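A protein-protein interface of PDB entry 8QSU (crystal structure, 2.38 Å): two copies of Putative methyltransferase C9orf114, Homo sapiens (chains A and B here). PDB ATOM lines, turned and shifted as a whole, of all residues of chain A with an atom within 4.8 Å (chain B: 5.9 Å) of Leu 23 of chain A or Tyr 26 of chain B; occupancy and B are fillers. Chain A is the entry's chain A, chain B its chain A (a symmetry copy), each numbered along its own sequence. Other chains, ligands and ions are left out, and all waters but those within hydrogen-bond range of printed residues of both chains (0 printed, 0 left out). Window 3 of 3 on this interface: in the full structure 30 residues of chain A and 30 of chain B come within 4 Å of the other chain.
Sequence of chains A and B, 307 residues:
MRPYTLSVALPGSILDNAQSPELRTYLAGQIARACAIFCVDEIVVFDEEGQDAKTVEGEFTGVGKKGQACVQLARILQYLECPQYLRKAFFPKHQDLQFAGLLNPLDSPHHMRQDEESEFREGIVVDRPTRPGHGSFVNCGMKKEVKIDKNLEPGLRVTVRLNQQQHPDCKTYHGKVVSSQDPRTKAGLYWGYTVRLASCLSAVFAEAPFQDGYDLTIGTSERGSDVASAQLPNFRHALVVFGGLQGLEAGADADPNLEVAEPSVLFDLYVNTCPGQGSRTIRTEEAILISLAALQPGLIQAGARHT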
ATOM      1  N   ALA A  18      26.140  10.806 -28.394  1.00  0.00           N
ATOM      2  CA  ALA A  18      24.742  10.470 -28.590  1.00  0.00           C
ATOM      3  C   ALA A  18      24.111  11.397 -29.628  1.00  0.00           C
ATOM      4  O   ALA A  18      24.565  12.522 -29.861  1.00  0.00           O
ATOM      5  CB  ALA A  18      23.981  10.533 -27.271  1.00  0.00           C
ATOM      6  N   GLN A  19      23.047  10.895 -30.262  1.00  0.00           N
ATOM      7  CA  GLN A  19      22.436  11.548 -31.412  1.00  0.00           C
ATOM      8  C   GLN A  19      21.278  12.462 -31.047  1.00  0.00           C
ATOM      9  O   GLN A  19      20.878  13.291 -31.872  1.00  0.00           O
ATOM     10  CB  GLN A  19      21.937  10.492 -32.408  1.00  0.00           C
ATOM     11  CG  GLN A  19      23.033   9.693 -33.077  1.00  0.00           C
ATOM     12  CD  GLN A  19      23.700  10.463 -34.197  1.00  0.00           C
ATOM     13  OE1 GLN A  19      24.912  10.356 -34.403  1.00  0.00           O
ATOM     14  NE2 GLN A  19      22.910  11.245 -34.934  1.00  0.00           N
ATOM     15  N   SER A  20      20.718  12.322 -29.849  1.00  0.00           N
ATOM     16  CA  SER A  20      19.610  13.158 -29.417  1.00  0.00           C
ATOM     17  C   SER A  20      19.678  13.271 -27.906  1.00  0.00           C
ATOM     18  O   SER A  20      20.189  12.357 -27.243  1.00  0.00           O
ATOM     19  CB  SER A  20      18.252  12.582 -29.847  1.00  0.00           C
ATOM     20  OG  SER A  20      17.739  11.698 -28.870  1.00  0.00           O
ATOM     21  N   PRO A  21      19.181  14.376 -27.327  1.00  0.00           N
ATOM     22  CA  PRO A  21      19.239  14.520 -25.860  1.00  0.00           C
ATOM     23  C   PRO A  21      18.590  13.363 -25.125  1.00  0.00           C
ATOM     24  O   PRO A  21      19.103  12.920 -24.094  1.00  0.00           O
ATOM     25  CB  PRO A  21      18.496  15.843 -25.602  1.00  0.00           C
ATOM     26  CG  PRO A  21      18.559  16.589 -26.885  1.00  0.00           C
ATOM     27  CD  PRO A  21      18.562  15.545 -27.983  1.00  0.00           C
ATOM     28  N   GLU A  22      17.465  12.862 -25.631  1.00  0.00           N
ATOM     29  CA  GLU A  22      16.848  11.674 -25.049  1.00  0.00           C
ATOM     30  C   GLU A  22      17.833  10.501 -25.007  1.00  0.00           C
ATOM     31  O   GLU A  22      18.058   9.891 -23.951  1.00  0.00           O
ATOM     32  CB  GLU A  22      15.593  11.311 -25.853  1.00  0.00           C
ATOM     33  CG  GLU A  22      14.575  12.448 -26.012  1.00  0.00           C
ATOM     34  CD  GLU A  22      14.801  13.308 -27.254  1.00  0.00           C
ATOM     35  OE1 GLU A  22      14.346  12.926 -28.367  1.00  0.00           O
ATOM     36  OE2 GLU A  22      15.428  14.375 -27.127  1.00  0.00           O
ATOM     37  N   LEU A  23      18.446  10.178 -26.150  1.00  0.00           N
ATOM     38  CA  LEU A  23      19.394   9.065 -26.189  1.00  0.00           C
ATOM     39  C   LEU A  23      20.590   9.311 -25.281  1.00  0.00           C
ATOM     40  O   LEU A  23      21.178   8.357 -24.752  1.00  0.00           O
ATOM     41  CB  LEU A  23      19.860   8.825 -27.624  1.00  0.00           C
ATOM     42  CG  LEU A  23      18.747   8.289 -28.501  1.00  0.00           C
ATOM     43  CD1 LEU A  23      19.048   8.550 -29.974  1.00  0.00           C
ATOM     44  CD2 LEU A  23      18.570   6.797 -28.215  1.00  0.00           C
ATOM     45  N   ARG A  24      20.980  10.577 -25.120  1.00  0.00           N
ATOM     46  CA  ARG A  24      22.015  10.941 -24.154  1.00  0.00           C
ATOM     47  C   ARG A  24      21.651  10.439 -22.770  1.00  0.00           C
ATOM     48  O   ARG A  24      22.441   9.749 -22.117  1.00  0.00           O
ATOM     49  CB  ARG A  24      22.187  12.455 -24.145  1.00  0.00           C
ATOM     50  CG  ARG A  24      23.468  12.944 -23.587  1.00  0.00           C
ATOM     51  CD  ARG A  24      23.472  14.451 -23.614  1.00  0.00           C
ATOM     52  NE  ARG A  24      24.743  14.942 -24.123  1.00  0.00           N
ATOM     53  CZ  ARG A  24      25.767  15.302 -23.361  1.00  0.00           C
ATOM     54  NH1 ARG A  24      25.685  15.296 -22.036  1.00  0.00           N
ATOM     55  NH2 ARG A  24      26.899  15.693 -23.944  1.00  0.00           N
ATOM     56  N   THR A  25      20.442  10.762 -22.315  1.00  0.00           N
ATOM     57  CA  THR A  25      19.932  10.221 -21.060  1.00  0.00           C
ATOM     58  C   THR A  25      19.866   8.700 -21.090  1.00  0.00           C
ATOM     59  O   THR A  25      20.320   8.028 -20.162  1.00  0.00           O
ATOM     60  CB  THR A  25      18.547  10.788 -20.795  1.00  0.00           C
ATOM     61  OG1 THR A  25      18.624  12.211 -20.762  1.00  0.00           O
ATOM     62  CG2 THR A  25      17.999  10.246 -19.485  1.00  0.00           C
ATOM     63  N   TYR A  26      19.255   8.139 -22.134  1.00  0.00           N
ATOM     64  CA  TYR A  26      19.054   6.696 -22.167  1.00  0.00           C
ATOM     65  C   TYR A  26      20.384   5.960 -22.078  1.00  0.00           C
ATOM     66  O   TYR A  26      20.523   5.000 -21.311  1.00  0.00           O
ATOM     67  CB  TYR A  26      18.288   6.323 -23.430  1.00  0.00           C
ATOM     68  CG  TYR A  26      17.830   4.892 -23.490  1.00  0.00           C
ATOM     69  CD1 TYR A  26      16.697   4.473 -22.799  1.00  0.00           C
ATOM     70  CD2 TYR A  26      18.517   3.969 -24.245  1.00  0.00           C
ATOM     71  CE1 TYR A  26      16.277   3.171 -22.849  1.00  0.00           C
ATOM     72  CE2 TYR A  26      18.104   2.677 -24.301  1.00  0.00           C
ATOM     73  CZ  TYR A  26      16.988   2.278 -23.599  1.00  0.00           C
ATOM     74  OH  TYR A  26      16.582   0.969 -23.684  1.00  0.00           O
ATOM     75  N   LEU A  27      21.391   6.433 -22.809  1.00  0.00           N
ATOM     76  CA  LEU A  27      22.721   5.847 -22.706  1.00  0.00           C
ATOM     77  C   LEU A  27      23.193   5.808 -21.253  1.00  0.00           C
ATOM     78  O   LEU A  27      23.614   4.761 -20.748  1.00  0.00           O
ATOM     79  CB  LEU A  27      23.697   6.645 -23.563  1.00  0.00           C
ATOM     80  CG  LEU A  27      25.134   6.138 -23.549  1.00  0.00           C
ATOM     81  CD1 LEU A  27      25.202   4.735 -24.132  1.00  0.00           C
ATOM     82  CD2 LEU A  27      26.023   7.102 -24.318  1.00  0.00           C
ATOM     83  N   GLN A  30      21.784   3.082 -19.500  1.00  0.00           N
ATOM     84  CA  GLN A  30      22.305   1.756 -19.842  1.00  0.00           C
ATOM     85  C   GLN A  30      23.580   1.472 -19.086  1.00  0.00           C
ATOM     86  O   GLN A  30      23.876   0.307 -18.809  1.00  0.00           O
ATOM     87  CB  GLN A  30      22.629   1.607 -21.339  1.00  0.00           C
ATOM     88  CG  GLN A  30      21.528   1.942 -22.287  1.00  0.00           C
ATOM     89  CD  GLN A  30      21.949   1.681 -23.718  1.00  0.00           C
ATOM     90  OE1 GLN A  30      22.190   2.614 -24.473  1.00  0.00           O
ATOM     91  NE2 GLN A  30      22.080   0.403 -24.083  1.00  0.00           N
ATOM     92  N   ARG A 283      30.757  -0.532 -28.840  1.00  0.00           N
ATOM     93  CA  ARG A 283      30.561   0.664 -28.045  1.00  0.00           C
ATOM     94  C   ARG A 283      30.722   0.347 -26.562  1.00  0.00           C
ATOM     95  O   ARG A 283      30.581  -0.806 -26.121  1.00  0.00           O
ATOM     96  CB  ARG A 283      29.192   1.261 -28.337  1.00  0.00           C
ATOM     97  CG  ARG A 283      28.937   1.355 -29.830  1.00  0.00           C
ATOM     98  CD  ARG A 283      27.464   1.513 -30.101  1.00  0.00           C
ATOM     99  NE  ARG A 283      26.933   2.647 -29.358  1.00  0.00           N
ATOM    100  CZ  ARG A 283      26.979   3.893 -29.804  1.00  0.00           C
ATOM    101  NH1 ARG A 283      27.478   4.173 -30.996  1.00  0.00           N
ATOM    102  NH2 ARG A 283      26.504   4.878 -29.040  1.00  0.00           N
ATOM    103  N   GLU A 285      29.021   1.011 -23.800  1.00  0.00           N
ATOM    104  CA  GLU A 285      27.916   0.386 -23.092  1.00  0.00           C
ATOM    105  C   GLU A 285      27.734  -1.074 -23.524  1.00  0.00           C
ATOM    106  O   GLU A 285      27.301  -1.905 -22.723  1.00  0.00           O
ATOM    107  CB  GLU A 285      26.644   1.208 -23.291  1.00  0.00           C
ATOM    108  CG  GLU A 285      25.929   1.039 -24.647  1.00  0.00           C
ATOM    109  CD  GLU A 285      26.428   1.977 -25.719  1.00  0.00           C
ATOM    110  OE1 GLU A 285      27.324   2.790 -25.393  1.00  0.00           O
ATOM    111  OE2 GLU A 285      25.922   1.897 -26.885  1.00  0.00           O
ATOM    112  N   PRO B  21       8.558   6.136 -29.721  1.00  0.00           N
ATOM    113  CA  PRO B  21       8.824   5.531 -31.039  1.00  0.00           C
ATOM    114  C   PRO B  21      10.297   5.515 -31.398  1.00  0.00           C
ATOM    115  O   PRO B  21      10.783   4.537 -31.973  1.00  0.00           O
ATOM    116  CB  PRO B  21       8.015   6.414 -32.006  1.00  0.00           C
ATOM    117  CG  PRO B  21       6.972   7.063 -31.172  1.00  0.00           C
ATOM    118  CD  PRO B  21       7.579   7.239 -29.795  1.00  0.00           C
ATOM    119  N   GLU B  22      11.024   6.583 -31.074  1.00  0.00           N
ATOM    120  CA  GLU B  22      12.469   6.594 -31.278  1.00  0.00           C
ATOM    121  C   GLU B  22      13.138   5.414 -30.564  1.00  0.00           C
ATOM    122  O   GLU B  22      13.889   4.638 -31.175  1.00  0.00           O
ATOM    123  CB  GLU B  22      13.039   7.930 -30.786  1.00  0.00           C
ATOM    124  CG  GLU B  22      12.381   9.177 -31.393  1.00  0.00           C
ATOM    125  CD  GLU B  22      11.187   9.694 -30.594  1.00  0.00           C
ATOM    126  OE1 GLU B  22      11.381  10.446 -29.599  1.00  0.00           O
ATOM    127  OE2 GLU B  22      10.045   9.359 -30.956  1.00  0.00           O
ATOM    128  N   LEU B  23      12.866   5.253 -29.265  1.00  0.00           N
ATOM    129  CA  LEU B  23      13.474   4.154 -28.516  1.00  0.00           C
ATOM    130  C   LEU B  23      13.059   2.798 -29.066  1.00  0.00           C
ATOM    131  O   LEU B  23      13.824   1.828 -28.978  1.00  0.00           O
ATOM    132  CB  LEU B  23      13.102   4.261 -27.038  1.00  0.00           C
ATOM    133  CG  LEU B  23      13.749   5.458 -26.373  1.00  0.00           C
ATOM    134  CD1 LEU B  23      12.989   5.851 -25.111  1.00  0.00           C
ATOM    135  CD2 LEU B  23      15.212   5.123 -26.072  1.00  0.00           C
ATOM    136  N   ARG B  24      11.841   2.708 -29.606  1.00  0.00           N
ATOM    137  CA  ARG B  24      11.400   1.501 -30.301  1.00  0.00           C
ATOM    138  C   ARG B  24      12.372   1.138 -31.407  1.00  0.00           C
ATOM    139  O   ARG B  24      12.863   0.007 -31.475  1.00  0.00           O
ATOM    140  CB  ARG B  24      10.004   1.726 -30.869  1.00  0.00           C
ATOM    141  CG  ARG B  24       9.243   0.498 -31.190  1.00  0.00           C
ATOM    142  CD  ARG B  24       7.908   0.884 -31.770  1.00  0.00           C
ATOM    143  NE  ARG B  24       6.848   0.094 -31.165  1.00  0.00           N
ATOM    144  CZ  ARG B  24       6.356  -1.023 -31.684  1.00  0.00           C
ATOM    145  NH1 ARG B  24       6.767  -1.486 -32.859  1.00  0.00           N
ATOM    146  NH2 ARG B  24       5.416  -1.687 -31.014  1.00  0.00           N
ATOM    147  N   THR B  25      12.676   2.101 -32.275  1.00  0.00           N
ATOM    148  CA  THR B  25      13.702   1.908 -33.295  1.00  0.00           C
ATOM    149  C   THR B  25      15.057   1.596 -32.676  1.00  0.00           C
ATOM    150  O   THR B  25      15.739   0.654 -33.085  1.00  0.00           O
ATOM    151  CB  THR B  25      13.806   3.164 -34.145  1.00  0.00           C
ATOM    152  OG1 THR B  25      12.533   3.441 -34.724  1.00  0.00           O
ATOM    153  CG2 THR B  25      14.862   2.984 -35.223  1.00  0.00           C
ATOM    154  N   TYR B  26      15.488   2.412 -31.714  1.00  0.00           N
ATOM    155  CA  TYR B  26      16.826   2.240 -31.161  1.00  0.00           C
ATOM    156  C   TYR B  26      16.993   0.848 -30.567  1.00  0.00           C
ATOM    157  O   TYR B  26      18.002   0.176 -30.809  1.00  0.00           O
ATOM    158  CB  TYR B  26      17.089   3.328 -30.128  1.00  0.00           C
ATOM    159  CG  TYR B  26      18.506   3.395 -29.630  1.00  0.00           C
ATOM    160  CD1 TYR B  26      19.502   4.009 -30.384  1.00  0.00           C
ATOM    161  CD2 TYR B  26      18.843   2.862 -28.407  1.00  0.00           C
ATOM    162  CE1 TYR B  26      20.795   4.071 -29.935  1.00  0.00           C
ATOM    163  CE2 TYR B  26      20.122   2.922 -27.955  1.00  0.00           C
ATOM    164  CZ  TYR B  26      21.097   3.522 -28.722  1.00  0.00           C
ATOM    165  OH  TYR B  26      22.380   3.584 -28.236  1.00  0.00           O
ATOM    166  N   LEU B  27      15.986   0.375 -29.836  1.00  0.00           N
ATOM    167  CA  LEU B  27      16.024  -0.985 -29.314  1.00  0.00           C
ATOM    168  C   LEU B  27      16.290  -1.995 -30.429  1.00  0.00           C
ATOM    169  O   LEU B  27      17.194  -2.832 -30.329  1.00  0.00           O
ATOM    170  CB  LEU B  27      14.708  -1.299 -28.612  1.00  0.00           C
ATOM    171  CG  LEU B  27      14.611  -2.697 -28.014  1.00  0.00           C
ATOM    172  CD1 LEU B  27      15.655  -2.876 -26.923  1.00  0.00           C
ATOM    173  CD2 LEU B  27      13.206  -2.928 -27.481  1.00  0.00           C
ATOM    174  N   ALA B  28      15.512  -1.912 -31.513  1.00  0.00           N
ATOM    175  CA  ALA B  28      15.699  -2.808 -32.650  1.00  0.00           C
ATOM    176  C   ALA B  28      17.136  -2.775 -33.139  1.00  0.00           C
ATOM    177  O   ALA B  28      17.719  -3.823 -33.432  1.00  0.00           O
ATOM    178  CB  ALA B  28      14.740  -2.421 -33.764  1.00  0.00           C
ATOM    179  N   GLY B  29      17.742  -1.580 -33.170  1.00  0.00           N
ATOM    180  CA  GLY B  29      19.144  -1.460 -33.532  1.00  0.00           C
ATOM    181  C   GLY B  29      20.080  -2.135 -32.552  1.00  0.00           C
ATOM    182  O   GLY B  29      21.133  -2.650 -32.951  1.00  0.00           O
ATOM    183  N   GLN B  30      19.722  -2.146 -31.259  1.00  0.00           N
ATOM    184  CA  GLN B  30      20.594  -2.801 -30.280  1.00  0.00           C
ATOM    185  C   GLN B  30      20.573  -4.298 -30.464  1.00  0.00           C
ATOM    186  O   GLN B  30      21.564  -4.964 -30.152  1.00  0.00           O
ATOM    187  CB  GLN B  30      20.179  -2.522 -28.825  1.00  0.00           C
ATOM    188  CG  GLN B  30      20.035  -1.087 -28.446  1.00  0.00           C
ATOM    189  CD  GLN B  30      19.699  -0.948 -26.976  1.00  0.00           C
ATOM    190  OE1 GLN B  30      18.572  -0.621 -26.625  1.00  0.00           O
ATOM    191  NE2 GLN B  30      20.672  -1.237 -26.107  1.00  0.00           N
ATOM    192  N   ILE B  31      19.429  -4.847 -30.897  1.00  0.00           N
ATOM    193  CA  ILE B  31      19.361  -6.283 -31.141  1.00  0.00           C
ATOM    194  C   ILE B  31      20.287  -6.656 -32.289  1.00  0.00           C
ATOM    195  O   ILE B  31      21.065  -7.612 -32.189  1.00  0.00           O
ATOM    196  CB  ILE B  31      17.904  -6.716 -31.403  1.00  0.00           C
ATOM    197  CG1 ILE B  31      17.020  -6.361 -30.189  1.00  0.00           C
ATOM    198  CG2 ILE B  31      17.831  -8.211 -31.709  1.00  0.00           C
ATOM    199  CD1 ILE B  31      17.288  -7.226 -28.933  1.00  0.00           C
ATOM    200  N   LEU B 102      18.692   7.657 -36.418  1.00  0.00           N
ATOM    201  CA  LEU B 102      19.122   7.582 -35.024  1.00  0.00           C
ATOM    202  C   LEU B 102      19.577   6.177 -34.650  1.00  0.00           C
ATOM    203  O   LEU B 102      19.416   5.757 -33.500  1.00  0.00           O
ATOM    204  CB  LEU B 102      17.986   8.016 -34.088  1.00  0.00           C
ATOM    205  CG  LEU B 102      17.275   9.355 -34.326  1.00  0.00           C
ATOM    206  CD1 LEU B 102      18.300  10.465 -34.521  1.00  0.00           C
ATOM    207  CD2 LEU B 102      16.283   9.284 -35.501  1.00  0.00           C
ATOM    208  N   LEU B 103      20.135   5.448 -35.609  1.00  0.00           N
ATOM    209  CA  LEU B 103      20.585   4.080 -35.407  1.00  0.00           C
ATOM    210  C   LEU B 103      22.092   4.046 -35.243  1.00  0.00           C
ATOM    211  O   LEU B 103      22.785   5.051 -35.405  1.00  0.00           O
ATOM    212  CB  LEU B 103      20.167   3.183 -36.585  1.00  0.00           C
ATOM    213  CG  LEU B 103      18.764   2.606 -36.439  1.00  0.00           C
ATOM    214  CD1 LEU B 103      18.215   2.156 -37.755  1.00  0.00           C
ATOM    215  CD2 LEU B 103      18.793   1.457 -35.456  1.00  0.00           C
ATOM    216  N   ASN B 104      22.591   2.852 -34.929  1.00  0.00           N
ATOM    217  CA  ASN B 104      24.014   2.584 -34.883  1.00  0.00           C
ATOM    218  C   ASN B 104      24.373   1.621 -36.006  1.00  0.00           C
ATOM    219  O   ASN B 104      23.846   0.500 -36.063  1.00  0.00           O
ATOM    220  CB  ASN B 104      24.416   2.020 -33.517  1.00  0.00           C
ATOM    221  CG  ASN B 104      24.211   3.031 -32.389  1.00  0.00           C
ATOM    222  OD1 ASN B 104      23.735   4.145 -32.635  1.00  0.00           O
ATOM    223  ND2 ASN B 104      24.558   2.651 -31.152  1.00  0.00           N
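Printed residues of chain B within 4 Å of Leu 23 of chain A: Tyr 26.
Printed residues of chain B within 4 Å of Gln 30 of chain A: Tyr 26 and Gln 30.
Of the printed residues of chain B, Arg 283 of chain A touches Asn 104.
Printed residues of chain A within 4 Å of Leu 23 of chain B: Tyr 26.
Printed residues of chain A within 4 Å of Tyr 26 of chain B: Leu 23 (3.7 Å) and Gln 30 (3.9 Å).
Ile 31 of chain B touches none of the printed residues of chain A.
Of the printed residues of chain A, Asn 104 of chain B touches Arg 283 (3.0 Å).
The nearest printed residue of chain A that does not touch Leu 23 of chain B is Leu 23 of chain A (4.3 Å).
CD1 of Tyr 26 of chain B touches CD2 of Leu 23 of chain A, at 3.7 Å.
CD1 of Tyr 26 of chain A touches CD2 of Leu 23 of chain B (3.7 Å).
Tyr 26 of chain A touches Gln 30 of chain B (OH to OE1, 3.9 Å).
Tyr 26 of chain B touches Gln 30 of chain A.
Leu 23 of chain A touches Tyr 26 of chain B, and with the chains exchanged Tyr 26 of chain A touches Leu 23 of chain B.
Tyr 26 of chain A touches Gln 30 of chain B, and with the chains exchanged Gln 30 of chain A touches Tyr 26 of chain B.
Gln 30 of chain B touches its own counterpart, Gln 30 of chain A.
8 positions are printed for both chains.
Of the 6 pairs that touch across the chains among the printed residues, 5 have their exchanged pair printed and touching as well.
The side-chain amide nitrogen of Gln 30 of chain B sits close to the side-chain amide nitrogen of Gln 30 of chain A.
NE of Arg 283 of chain A sits close to ND2 of Asn 104 of chain B (3.0 Å).
Printed residues of chain A that touch a printed residue of chain B: Leu 23, Tyr 26, Gln 30 and Arg 283.
The side-chain hydroxyl of Ser 20 of chain A sits at hydrogen-bond distance from the backbone NH of Leu 23 of chain A (3.2 Å).
The guanidinium group (NE) of Arg 283 of chain A lies within salt-bridge range of the side-chain carboxylate (OE2) of Glu 285 of chain A (2.8 Å).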
